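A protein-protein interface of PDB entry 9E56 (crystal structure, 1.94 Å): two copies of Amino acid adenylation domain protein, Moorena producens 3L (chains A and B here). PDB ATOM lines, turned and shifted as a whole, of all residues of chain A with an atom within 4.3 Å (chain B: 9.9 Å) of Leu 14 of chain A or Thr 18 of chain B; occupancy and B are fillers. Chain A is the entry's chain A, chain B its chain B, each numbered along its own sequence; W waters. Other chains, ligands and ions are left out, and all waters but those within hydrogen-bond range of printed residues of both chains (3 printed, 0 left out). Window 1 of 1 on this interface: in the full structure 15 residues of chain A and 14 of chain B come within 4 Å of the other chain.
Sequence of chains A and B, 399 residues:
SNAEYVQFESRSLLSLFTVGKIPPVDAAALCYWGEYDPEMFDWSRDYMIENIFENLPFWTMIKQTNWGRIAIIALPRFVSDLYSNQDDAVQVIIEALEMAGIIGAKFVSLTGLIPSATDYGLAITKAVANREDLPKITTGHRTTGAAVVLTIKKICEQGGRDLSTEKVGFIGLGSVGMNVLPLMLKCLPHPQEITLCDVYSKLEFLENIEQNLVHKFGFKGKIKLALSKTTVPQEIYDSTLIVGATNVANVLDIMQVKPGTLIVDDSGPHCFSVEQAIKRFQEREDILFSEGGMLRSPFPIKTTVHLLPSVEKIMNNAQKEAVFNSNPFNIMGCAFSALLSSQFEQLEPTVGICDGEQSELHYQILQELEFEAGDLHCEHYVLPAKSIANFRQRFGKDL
O of Thr 18 of chain A is in hydrogen-bond range of N of Met 99 of chain B, at 3.2 Å.
O of Thr 18 of chain B sits at hydrogen-bond distance from N of Met 99 of chain A (3.4 Å).
The side-chain hydroxyl (OG) of Ser 12 of chain A sits close to the backbone NH (N) of Leu 14 of chain A, at 3.3 Å.
The side-chain hydroxyl (OG) of Ser 12 of chain A lies within hydrogen-bond range of the backbone NH (N) of Ser 15 of chain A (3.3 Å).
O of Ser 15 of chain A is in hydrogen-bond range of OG1 of Thr 18 of chain A, 2.9 Å away.
OG of Ser 12 of chain B lies close to N of Leu 14 of chain B, at 3.2 Å.
OG of Ser 12 of chain B lies within hydrogen-bond range of N of Ser 15 of chain B (3.1 Å).
The side-chain hydroxyl (OG1) of Thr 18 of chain B lies within hydrogen-bond range of the backbone carbonyl oxygen (O) of Ser 15 of chain B (2.9 Å).
Leu 14 of chain A touches Ser 15 of chain B.
Leu 14 of chain A touches Thr 18 of chain B (CD2 to OG1, 3.7 Å).
CD2 of Leu 14 of chain B touches OG of Ser 15 of chain A, 3.8 Å away.
Ser 15 of chain A touches Leu 56 of chain B.
Leu 14 of chain B touches Thr 18 of chain A (CD2 to OG1, 3.7 Å).
Thr 18 of chain A touches Ile 102 of chain B.
CG of Glu 98 of chain A touches O of Thr 18 of chain B, at 3.5 Å.
OE1 of Glu 98 of chain A touches O of Val 19 of chain B, at 3.9 Å.
CA of Gly 20 of chain B touches OE2 of Glu 98 of chain A, at 3.4 Å.
Thr 18 of chain B touches Ile 102 of chain A (O to CD1, 3.7 Å).
Printed residues of chain B within 4 Å of Leu 14 of chain A: Ser 15 and Thr 18.
Thr 18 of chain B touches four residues of chain A.
Ser 15 of chain A touches two residues of chain B.
Glu 98 of chain A touches just these residues of chain B: Thr 18, Val 19 and Gly 20.
Met 99 of chain A touches just one residue of chain B: Thr 18.
Printed residues of chain A within 4 Å of Leu 14 of chain B: Ser 15 (3.8 Å) and Thr 18 (3.7 Å).
Of the printed residues of chain A, Ser 15 of chain B touches Leu 14 (3.8 Å).
Of the printed residues of chain B, Ile 102 of chain A touches Thr 18 (3.7 Å).
Printed residues of chain A within 4 Å of Val 19 of chain B: Glu 98 (3.9 Å).
Of the printed residues of chain A, Glu 98 of chain B touches Thr 18.
Ile 103 of chain B touches none of the printed residues of chain A.
The nearest residue of chain B that does not touch Leu 14 of chain A is Leu 14 of chain B (4.2 Å).
The nearest printed residue of chain A that does not touch Glu 98 of chain B is Phe 17 of chain A (4.3 Å).
Of the 22 printed residues of chain B, 9 touch a printed residue of chain A.
Hydrophobic or aromatic side chains of chain B that line the printed part of chain A: Leu 14, Leu 56, Met 99 and Ile 102.
Printed residues of chain A that touch a printed residue of chain B: Leu 14, Ser 15, Thr 18, Glu 98, Met 99 and Ile 102.
Hydrophobic or aromatic side chains of chain A that line the printed part of chain B: Leu 14, Met 99 and Ile 102.
Among the printed residues, no Asp or Glu carboxylate lies within 4 Å of a Lys or Arg side-chain nitrogen of the other chain.
Leu 14 of chain A touches Ser 15 of chain B, and with the chains exchanged Ser 15 of chain A touches Leu 14 of chain B.
Leu 14 of chain A touches Thr 18 of chain B, and with the chains exchanged Thr 18 of chain A touches Leu 14 of chain B.
Thr 18 of chain A touches Met 99 of chain B, and with the chains exchanged Met 99 of chain A touches Thr 18 of chain B.
Thr 18 of chain A touches Ile 102 of chain B, and with the chains exchanged Ile 102 of chain A touches Thr 18 of chain B.
Water W2 lies within hydrogen-bond range of O of Phe 17 of chain A (2.6 Å) and OE2 of Glu 98 of chain B (2.7 Å).
Water W1 bridges O of Phe 17 of chain B (2.7 Å) and OE2 of Glu 98 of chain A (2.9 Å).
Water W3 lies within hydrogen-bond range of O of Pro 57 of chain B (2.8 Å) and OG of Ser 15 of chain A (3.1 Å).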
ATOM      1  N   SER A  12      16.252  35.169 -28.121  1.00  0.00           N
ATOM      2  CA  SER A  12      16.503  33.770 -28.446  1.00  0.00           C
ATOM      3  C   SER A  12      15.714  32.841 -27.539  1.00  0.00           C
ATOM      4  O   SER A  12      15.802  32.929 -26.309  1.00  0.00           O
ATOM      5  CB  SER A  12      18.001  33.483 -28.322  1.00  0.00           C
ATOM      6  OG  SER A  12      18.267  32.100 -28.385  1.00  0.00           O
ATOM      7  N   LEU A  13      14.939  31.938 -28.153  1.00  0.00           N
ATOM      8  CA  LEU A  13      14.210  30.940 -27.379  1.00  0.00           C
ATOM      9  C   LEU A  13      15.168  30.049 -26.601  1.00  0.00           C
ATOM     10  O   LEU A  13      14.889  29.672 -25.457  1.00  0.00           O
ATOM     11  CB  LEU A  13      13.328  30.097 -28.305  1.00  0.00           C
ATOM     12  CG  LEU A  13      12.230  30.858 -29.056  1.00  0.00           C
ATOM     13  CD1 LEU A  13      11.332  29.896 -29.852  1.00  0.00           C
ATOM     14  CD2 LEU A  13      11.406  31.703 -28.071  1.00  0.00           C
ATOM     15  N   LEU A  14      16.309  29.704 -27.201  1.00  0.00           N
ATOM     16  CA  LEU A  14      17.264  28.843 -26.505  1.00  0.00           C
ATOM     17  C   LEU A  14      17.815  29.531 -25.267  1.00  0.00           C
ATOM     18  O   LEU A  14      17.922  28.909 -24.202  1.00  0.00           O
ATOM     19  CB  LEU A  14      18.400  28.434 -27.443  1.00  0.00           C
ATOM     20  CG  LEU A  14      19.459  27.485 -26.874  1.00  0.00           C
ATOM     21  CD1 LEU A  14      18.823  26.145 -26.493  1.00  0.00           C
ATOM     22  CD2 LEU A  14      20.565  27.279 -27.900  1.00  0.00           C
ATOM     23  N   SER A  15      18.160  30.816 -25.382  1.00  0.00           N
ATOM     24  CA  SER A  15      18.657  31.560 -24.227  1.00  0.00           C
ATOM     25  C   SER A  15      17.604  31.644 -23.131  1.00  0.00           C
ATOM     26  O   SER A  15      17.904  31.428 -21.953  1.00  0.00           O
ATOM     27  CB  SER A  15      19.091  32.960 -24.655  1.00  0.00           C
ATOM     28  OG  SER A  15      20.234  32.891 -25.483  1.00  0.00           O
ATOM     29  N   LEU A  16      16.362  31.956 -23.505  1.00  0.00           N
ATOM     30  CA  LEU A  16      15.290  32.054 -22.520  1.00  0.00           C
ATOM     31  C   LEU A  16      15.048  30.722 -21.833  1.00  0.00           C
ATOM     32  O   LEU A  16      14.752  30.683 -20.633  1.00  0.00           O
ATOM     33  CB  LEU A  16      14.002  32.541 -23.184  1.00  0.00           C
ATOM     34  CG  LEU A  16      14.023  33.950 -23.771  1.00  0.00           C
ATOM     35  CD1 LEU A  16      12.841  34.121 -24.696  1.00  0.00           C
ATOM     36  CD2 LEU A  16      13.985  34.980 -22.659  1.00  0.00           C
ATOM     37  N   PHE A  17      15.174  29.614 -22.577  1.00  0.00           N
ATOM     38  CA  PHE A  17      15.028  28.307 -21.951  1.00  0.00           C
ATOM     39  C   PHE A  17      16.129  28.050 -20.930  1.00  0.00           C
ATOM     40  O   PHE A  17      15.867  27.507 -19.845  1.00  0.00           O
ATOM     41  CB  PHE A  17      15.032  27.183 -22.991  1.00  0.00           C
ATOM     42  CG  PHE A  17      15.215  25.826 -22.372  1.00  0.00           C
ATOM     43  CD1 PHE A  17      14.142  25.169 -21.789  1.00  0.00           C
ATOM     44  CD2 PHE A  17      16.470  25.240 -22.309  1.00  0.00           C
ATOM     45  CE1 PHE A  17      14.306  23.943 -21.180  1.00  0.00           C
ATOM     46  CE2 PHE A  17      16.639  24.014 -21.696  1.00  0.00           C
ATOM     47  CZ  PHE A  17      15.560  23.363 -21.130  1.00  0.00           C
ATOM     48  N   THR A  18      17.376  28.389 -21.273  1.00  0.00           N
ATOM     49  CA  THR A  18      18.492  28.012 -20.405  1.00  0.00           C
ATOM     50  C   THR A  18      18.524  28.802 -19.096  1.00  0.00           C
ATOM     51  O   THR A  18      19.152  28.342 -18.137  1.00  0.00           O
ATOM     52  CB  THR A  18      19.838  28.155 -21.137  1.00  0.00           C
ATOM     53  OG1 THR A  18      20.080  29.520 -21.492  1.00  0.00           O
ATOM     54  CG2 THR A  18      19.850  27.315 -22.390  1.00  0.00           C
ATOM     55  N   TRP A  59      16.005  27.086 -33.338  1.00  0.00           N
ATOM     56  CA  TRP A  59      14.717  26.930 -32.666  1.00  0.00           C
ATOM     57  C   TRP A  59      13.894  28.190 -32.902  1.00  0.00           C
ATOM     58  O   TRP A  59      14.181  29.249 -32.332  1.00  0.00           O
ATOM     59  CB  TRP A  59      14.947  26.678 -31.182  1.00  0.00           C
ATOM     60  CG  TRP A  59      13.713  26.477 -30.378  1.00  0.00           C
ATOM     61  CD1 TRP A  59      12.434  26.321 -30.832  1.00  0.00           C
ATOM     62  CD2 TRP A  59      13.647  26.425 -28.958  1.00  0.00           C
ATOM     63  NE1 TRP A  59      11.572  26.167 -29.773  1.00  0.00           N
ATOM     64  CE2 TRP A  59      12.297  26.222 -28.609  1.00  0.00           C
ATOM     65  CE3 TRP A  59      14.607  26.510 -27.942  1.00  0.00           C
ATOM     66  CZ2 TRP A  59      11.880  26.095 -27.284  1.00  0.00           C
ATOM     67  CZ3 TRP A  59      14.185  26.403 -26.617  1.00  0.00           C
ATOM     68  CH2 TRP A  59      12.836  26.200 -26.303  1.00  0.00           C
ATOM     69  N   GLU A  98      20.265  16.592 -30.586  1.00  0.00           N
ATOM     70  CA  GLU A  98      20.915  16.902 -29.319  1.00  0.00           C
ATOM     71  C   GLU A  98      20.338  18.173 -28.704  1.00  0.00           C
ATOM     72  O   GLU A  98      20.096  18.225 -27.491  1.00  0.00           O
ATOM     73  CB  GLU A  98      22.429  17.028 -29.505  1.00  0.00           C
ATOM     74  CG  GLU A  98      23.177  17.063 -28.168  1.00  0.00           C
ATOM     75  CD  GLU A  98      24.671  16.776 -28.298  1.00  0.00           C
ATOM     76  OE1 GLU A  98      25.058  16.026 -29.224  1.00  0.00           O
ATOM     77  OE2 GLU A  98      25.453  17.304 -27.467  1.00  0.00           O
ATOM     78  N   MET A  99      20.090  19.199 -29.523  1.00  0.00           N
ATOM     79  CA  MET A  99      19.465  20.411 -29.009  1.00  0.00           C
ATOM     80  C   MET A  99      18.043  20.125 -28.532  1.00  0.00           C
ATOM     81  O   MET A  99      17.643  20.547 -27.434  1.00  0.00           O
ATOM     82  CB  MET A  99      19.480  21.510 -30.077  1.00  0.00           C
ATOM     83  CG  MET A  99      18.592  22.728 -29.741  1.00  0.00           C
ATOM     84  SD  MET A  99      18.483  23.985 -31.060  1.00  0.00           S
ATOM     85  CE  MET A  99      20.111  24.709 -30.970  1.00  0.00           C
ATOM     86  N   ILE A 102      18.056  18.555 -25.101  1.00  0.00           N
ATOM     87  CA  ILE A 102      18.376  19.488 -24.025  1.00  0.00           C
ATOM     88  C   ILE A 102      17.150  20.310 -23.628  1.00  0.00           C
ATOM     89  O   ILE A 102      16.936  20.584 -22.440  1.00  0.00           O
ATOM     90  CB  ILE A 102      19.561  20.378 -24.435  1.00  0.00           C
ATOM     91  CG1 ILE A 102      20.855  19.566 -24.355  1.00  0.00           C
ATOM     92  CG2 ILE A 102      19.650  21.620 -23.553  1.00  0.00           C
ATOM     93  CD1 ILE A 102      22.034  20.232 -25.000  1.00  0.00           C
ATOM     94  N   ILE A 103      16.310  20.690 -24.596  1.00  0.00           N
ATOM     95  CA  ILE A 103      15.171  21.547 -24.274  1.00  0.00           C
ATOM     96  C   ILE A 103      13.942  20.725 -23.891  1.00  0.00           C
ATOM     97  O   ILE A 103      12.860  21.282 -23.666  1.00  0.00           O
ATOM     98  CB  ILE A 103      14.852  22.526 -25.424  1.00  0.00           C
ATOM     99  CG1 ILE A 103      14.385  21.789 -26.682  1.00  0.00           C
ATOM    100  CG2 ILE A 103      16.061  23.406 -25.690  1.00  0.00           C
ATOM    101  CD1 ILE A 103      13.892  22.708 -27.797  1.00  0.00           C
ATOM    102  N   SER B  12      27.152  31.885 -31.444  1.00  0.00           N
ATOM    103  CA  SER B  12      26.852  31.746 -30.023  1.00  0.00           C
ATOM    104  C   SER B  12      27.499  30.499 -29.436  1.00  0.00           C
ATOM    105  O   SER B  12      27.283  29.380 -29.920  1.00  0.00           O
ATOM    106  CB  SER B  12      25.337  31.698 -29.823  1.00  0.00           C
ATOM    107  OG  SER B  12      24.995  31.254 -28.520  1.00  0.00           O
ATOM    108  N   LEU B  13      28.297  30.698 -28.387  1.00  0.00           N
ATOM    109  CA  LEU B  13      28.846  29.566 -27.653  1.00  0.00           C
ATOM    110  C   LEU B  13      27.735  28.678 -27.110  1.00  0.00           C
ATOM    111  O   LEU B  13      27.863  27.451 -27.106  1.00  0.00           O
ATOM    112  CB  LEU B  13      29.748  30.061 -26.521  1.00  0.00           C
ATOM    113  CG  LEU B  13      30.926  30.937 -26.947  1.00  0.00           C
ATOM    114  CD1 LEU B  13      31.742  31.394 -25.740  1.00  0.00           C
ATOM    115  CD2 LEU B  13      31.809  30.192 -27.949  1.00  0.00           C
ATOM    116  N   LEU B  14      26.626  29.277 -26.663  1.00  0.00           N
ATOM    117  CA  LEU B  14      25.522  28.476 -26.149  1.00  0.00           C
ATOM    118  C   LEU B  14      24.947  27.577 -27.243  1.00  0.00           C
ATOM    119  O   LEU B  14      24.691  26.390 -27.013  1.00  0.00           O
ATOM    120  CB  LEU B  14      24.444  29.386 -25.558  1.00  0.00           C
ATOM    121  CG  LEU B  14      23.236  28.700 -24.911  1.00  0.00           C
ATOM    122  CD1 LEU B  14      23.669  27.937 -23.681  1.00  0.00           C
ATOM    123  CD2 LEU B  14      22.140  29.711 -24.553  1.00  0.00           C
ATOM    124  N   SER B  15      24.750  28.121 -28.443  1.00  0.00           N
ATOM    125  CA  SER B  15      24.256  27.307 -29.552  1.00  0.00           C
ATOM    126  C   SER B  15      25.229  26.187 -29.899  1.00  0.00           C
ATOM    127  O   SER B  15      24.827  25.030 -30.079  1.00  0.00           O
ATOM    128  CB  SER B  15      24.010  28.192 -30.767  1.00  0.00           C
ATOM    129  OG  SER B  15      22.760  28.834 -30.654  1.00  0.00           O
ATOM    130  N   LEU B  16      26.520  26.515 -29.984  1.00  0.00           N
ATOM    131  CA  LEU B  16      27.527  25.514 -30.322  1.00  0.00           C
ATOM    132  C   LEU B  16      27.578  24.404 -29.281  1.00  0.00           C
ATOM    133  O   LEU B  16      27.757  23.226 -29.622  1.00  0.00           O
ATOM    134  CB  LEU B  16      28.894  26.186 -30.463  1.00  0.00           C
ATOM    135  CG  LEU B  16      29.085  27.046 -31.706  1.00  0.00           C
ATOM    136  CD1 LEU B  16      30.308  27.915 -31.521  1.00  0.00           C
ATOM    137  CD2 LEU B  16      29.268  26.145 -32.917  1.00  0.00           C
ATOM    138  N   PHE B  17      27.410  24.754 -28.003  1.00  0.00           N
ATOM    139  CA  PHE B  17      27.383  23.729 -26.968  1.00  0.00           C
ATOM    140  C   PHE B  17      26.186  22.802 -27.130  1.00  0.00           C
ATOM    141  O   PHE B  17      26.306  21.585 -26.941  1.00  0.00           O
ATOM    142  CB  PHE B  17      27.357  24.358 -25.569  1.00  0.00           C
ATOM    143  CG  PHE B  17      26.924  23.390 -24.504  1.00  0.00           C
ATOM    144  CD1 PHE B  17      27.841  22.512 -23.939  1.00  0.00           C
ATOM    145  CD2 PHE B  17      25.601  23.320 -24.104  1.00  0.00           C
ATOM    146  CE1 PHE B  17      27.448  21.597 -22.994  1.00  0.00           C
ATOM    147  CE2 PHE B  17      25.203  22.403 -23.160  1.00  0.00           C
ATOM    148  CZ  PHE B  17      26.123  21.546 -22.595  1.00  0.00           C
ATOM    149  N   THR B  18      25.007  23.355 -27.435  1.00  0.00           N
ATOM    150  CA  THR B  18      23.812  22.516 -27.420  1.00  0.00           C
ATOM    151  C   THR B  18      23.760  21.549 -28.597  1.00  0.00           C
ATOM    152  O   THR B  18      22.988  20.585 -28.550  1.00  0.00           O
ATOM    153  CB  THR B  18      22.528  23.354 -27.404  1.00  0.00           C
ATOM    154  OG1 THR B  18      22.454  24.152 -28.589  1.00  0.00           O
ATOM    155  CG2 THR B  18      22.486  24.254 -26.187  1.00  0.00           C
ATOM    156  N   VAL B  19      24.544  21.772 -29.652  1.00  0.00           N
ATOM    157  CA  VAL B  19      24.626  20.792 -30.733  1.00  0.00           C
ATOM    158  C   VAL B  19      25.839  19.885 -30.583  1.00  0.00           C
ATOM    159  O   VAL B  19      26.111  19.071 -31.471  1.00  0.00           O
ATOM    160  CB  VAL B  19      24.613  21.465 -32.117  1.00  0.00           C
ATOM    161  CG1 VAL B  19      23.341  22.283 -32.282  1.00  0.00           C
ATOM    162  CG2 VAL B  19      25.849  22.332 -32.327  1.00  0.00           C
ATOM    163  N   GLY B  20      26.581  20.013 -29.486  1.00  0.00           N
ATOM    164  CA  GLY B  20      27.724  19.167 -29.238  1.00  0.00           C
ATOM    165  C   GLY B  20      28.998  19.570 -29.940  1.00  0.00           C
ATOM    166  O   GLY B  20      29.934  18.766 -29.994  1.00  0.00           O
ATOM    167  N   LYS B  21      29.070  20.775 -30.494  1.00  0.00           N
ATOM    168  CA  LYS B  21      30.293  21.217 -31.150  1.00  0.00           C
ATOM    169  C   LYS B  21      31.293  21.829 -30.183  1.00  0.00           C
ATOM    170  O   LYS B  21      32.452  22.021 -30.560  1.00  0.00           O
ATOM    171  CB  LYS B  21      29.965  22.219 -32.261  1.00  0.00           C
ATOM    172  CG  LYS B  21      29.205  21.576 -33.426  1.00  0.00           C
ATOM    173  CD  LYS B  21      28.997  22.528 -34.589  1.00  0.00           C
ATOM    174  CE  LYS B  21      28.336  21.797 -35.759  1.00  0.00           C
ATOM    175  NZ  LYS B  21      28.012  22.710 -36.891  1.00  0.00           N
ATOM    176  N   ILE B  22      30.865  22.146 -28.966  1.00  0.00           N
ATOM    177  CA  ILE B  22      31.729  22.641 -27.901  1.00  0.00           C
ATOM    178  C   ILE B  22      31.550  21.700 -26.719  1.00  0.00           C
ATOM    179  O   ILE B  22      30.413  21.416 -26.338  1.00  0.00           O
ATOM    180  CB  ILE B  22      31.374  24.083 -27.486  1.00  0.00           C
ATOM    181  CG1 ILE B  22      31.882  25.098 -28.500  1.00  0.00           C
ATOM    182  CG2 ILE B  22      31.907  24.431 -26.101  1.00  0.00           C
ATOM    183  CD1 ILE B  22      31.556  26.533 -28.071  1.00  0.00           C
ATOM    184  N   PRO B  23      32.619  21.183 -26.121  1.00  0.00           N
ATOM    185  CA  PRO B  23      32.469  20.318 -24.949  1.00  0.00           C
ATOM    186  C   PRO B  23      31.936  21.105 -23.763  1.00  0.00           C
ATOM    187  O   PRO B  23      32.099  22.331 -23.704  1.00  0.00           O
ATOM    188  CB  PRO B  23      33.901  19.826 -24.683  1.00  0.00           C
ATOM    189  CG  PRO B  23      34.682  20.147 -25.931  1.00  0.00           C
ATOM    190  CD  PRO B  23      34.028  21.337 -26.530  1.00  0.00           C
ATOM    191  N   PRO B  24      31.303  20.445 -22.794  1.00  0.00           N
ATOM    192  CA  PRO B  24      30.908  21.150 -21.568  1.00  0.00           C
ATOM    193  C   PRO B  24      32.115  21.752 -20.863  1.00  0.00           C
ATOM    194  O   PRO B  24      33.270  21.428 -21.153  1.00  0.00           O
ATOM    195  CB  PRO B  24      30.251  20.058 -20.714  1.00  0.00           C
ATOM    196  CG  PRO B  24      30.663  18.745 -21.353  1.00  0.00           C
ATOM    197  CD  PRO B  24      30.865  19.039 -22.800  1.00  0.00           C
ATOM    198  N   LEU B  56      19.623  39.207 -20.409  1.00  0.00           N
ATOM    199  CA  LEU B  56      20.028  37.815 -20.342  1.00  0.00           C
ATOM    200  C   LEU B  56      21.517  37.724 -20.050  1.00  0.00           C
ATOM    201  O   LEU B  56      22.294  38.576 -20.494  1.00  0.00           O
ATOM    202  CB  LEU B  56      19.712  37.080 -21.656  1.00  0.00           C
ATOM    203  CG  LEU B  56      18.236  36.873 -21.996  1.00  0.00           C
ATOM    204  CD1 LEU B  56      18.047  36.516 -23.459  1.00  0.00           C
ATOM    205  CD2 LEU B  56      17.625  35.800 -21.102  1.00  0.00           C
ATOM    206  N   PRO B  57      21.940  36.716 -19.291  1.00  0.00           N
ATOM    207  CA  PRO B  57      23.374  36.444 -19.184  1.00  0.00           C
ATOM    208  C   PRO B  57      23.933  36.109 -20.557  1.00  0.00           C
ATOM    209  O   PRO B  57      23.224  35.605 -21.432  1.00  0.00           O
ATOM    210  CB  PRO B  57      23.445  35.245 -18.231  1.00  0.00           C
ATOM    211  CG  PRO B  57      22.104  34.612 -18.313  1.00  0.00           C
ATOM    212  CD  PRO B  57      21.125  35.721 -18.577  1.00  0.00           C
ATOM    213  N   TRP B  59      27.160  34.274 -22.404  1.00  0.00           N
ATOM    214  CA  TRP B  59      28.345  33.431 -22.369  1.00  0.00           C
ATOM    215  C   TRP B  59      29.327  33.946 -23.413  1.00  0.00           C
ATOM    216  O   TRP B  59      29.109  33.784 -24.622  1.00  0.00           O
ATOM    217  CB  TRP B  59      27.949  31.982 -22.617  1.00  0.00           C
ATOM    218  CG  TRP B  59      29.074  31.024 -22.547  1.00  0.00           C
ATOM    219  CD1 TRP B  59      30.359  31.278 -22.153  1.00  0.00           C
ATOM    220  CD2 TRP B  59      29.025  29.646 -22.892  1.00  0.00           C
ATOM    221  NE1 TRP B  59      31.112  30.133 -22.238  1.00  0.00           N
ATOM    222  CE2 TRP B  59      30.311  29.115 -22.686  1.00  0.00           C
ATOM    223  CE3 TRP B  59      28.014  28.801 -23.365  1.00  0.00           C
ATOM    224  CZ2 TRP B  59      30.611  27.779 -22.935  1.00  0.00           C
ATOM    225  CZ3 TRP B  59      28.316  27.482 -23.606  1.00  0.00           C
ATOM    226  CH2 TRP B  59      29.599  26.982 -23.390  1.00  0.00           C
ATOM    227  N   GLU B  95      19.583  33.307 -12.567  1.00  0.00           N
ATOM    228  CA  GLU B  95      19.345  32.978 -13.969  1.00  0.00           C
ATOM    229  C   GLU B  95      20.632  32.542 -14.658  1.00  0.00           C
ATOM    230  O   GLU B  95      20.626  31.620 -15.481  1.00  0.00           O
ATOM    231  CB  GLU B  95      18.737  34.174 -14.700  1.00  0.00           C
ATOM    232  CG  GLU B  95      17.300  34.467 -14.303  1.00  0.00           C
ATOM    233  CD  GLU B  95      16.761  35.733 -14.940  1.00  0.00           C
ATOM    234  OE1 GLU B  95      17.493  36.371 -15.734  1.00  0.00           O
ATOM    235  OE2 GLU B  95      15.598  36.088 -14.642  1.00  0.00           O
ATOM    236  N   GLU B  98      21.598  28.926 -13.604  1.00  0.00           N
ATOM    237  CA  GLU B  98      20.886  27.863 -14.309  1.00  0.00           C
ATOM    238  C   GLU B  98      21.537  27.570 -15.659  1.00  0.00           C
ATOM    239  O   GLU B  98      21.776  26.406 -16.003  1.00  0.00           O
ATOM    240  CB  GLU B  98      19.415  28.241 -14.482  1.00  0.00           C
ATOM    241  CG  GLU B  98      18.577  27.151 -15.120  1.00  0.00           C
ATOM    242  CD  GLU B  98      17.088  27.369 -14.923  1.00  0.00           C
ATOM    243  OE1 GLU B  98      16.716  28.189 -14.052  1.00  0.00           O
ATOM    244  OE2 GLU B  98      16.292  26.719 -15.638  1.00  0.00           O
ATOM    245  N   MET B  99      21.846  28.618 -16.429  1.00  0.00           N
ATOM    246  CA  MET B  99      22.617  28.435 -17.655  1.00  0.00           C
ATOM    247  C   MET B  99      23.946  27.745 -17.372  1.00  0.00           C
ATOM    248  O   MET B  99      24.316  26.786 -18.060  1.00  0.00           O
ATOM    249  CB  MET B  99      22.863  29.779 -18.331  1.00  0.00           C
ATOM    250  CG  MET B  99      23.718  29.649 -19.595  1.00  0.00           C
ATOM    251  SD  MET B  99      24.237  31.227 -20.291  1.00  0.00           S
ATOM    252  CE  MET B  99      22.716  31.749 -21.080  1.00  0.00           C
ATOM    253  N   ILE B 102      23.634  24.134 -16.944  1.00  0.00           N
ATOM    254  CA  ILE B 102      23.308  23.417 -18.173  1.00  0.00           C
ATOM    255  C   ILE B 102      24.565  23.152 -18.995  1.00  0.00           C
ATOM    256  O   ILE B 102      24.722  22.071 -19.580  1.00  0.00           O
ATOM    257  CB  ILE B 102      22.245  24.197 -18.971  1.00  0.00           C
ATOM    258  CG1 ILE B 102      20.857  24.001 -18.347  1.00  0.00           C
ATOM    259  CG2 ILE B 102      22.238  23.776 -20.433  1.00  0.00           C
ATOM    260  CD1 ILE B 102      19.818  24.912 -18.922  1.00  0.00           C
ATOM    261  N   ILE B 103      25.493  24.118 -19.041  1.00  0.00           N
ATOM    262  CA  ILE B 103      26.697  23.965 -19.856  1.00  0.00           C
ATOM    263  C   ILE B 103      27.815  23.227 -19.129  1.00  0.00           C
ATOM    264  O   ILE B 103      28.909  23.092 -19.688  1.00  0.00           O
ATOM    265  CB  ILE B 103      27.207  25.329 -20.380  1.00  0.00           C
ATOM    266  CG1 ILE B 103      27.689  26.241 -19.242  1.00  0.00           C
ATOM    267  CG2 ILE B 103      26.129  26.034 -21.213  1.00  0.00           C
ATOM    268  CD1 ILE B 103      28.310  27.518 -19.742  1.00  0.00           C
ATOM    269  N   GLY B 104      27.579  22.740 -17.911  1.00  0.00           N
ATOM    270  CA  GLY B 104      28.476  21.801 -17.255  1.00  0.00           C
ATOM    271  C   GLY B 104      29.103  22.274 -15.959  1.00  0.00           C
ATOM    272  O   GLY B 104      29.654  21.444 -15.227  1.00  0.00           O
HETATM  273  O   HOH W   1      25.879  19.359 -25.503  1.00  0.00           O
HETATM  274  O   HOH W   2      16.257  25.607 -18.132  1.00  0.00           O
HETATM  275  O   HOH W   3      22.415  33.981 -23.559  1.00  0.00           O
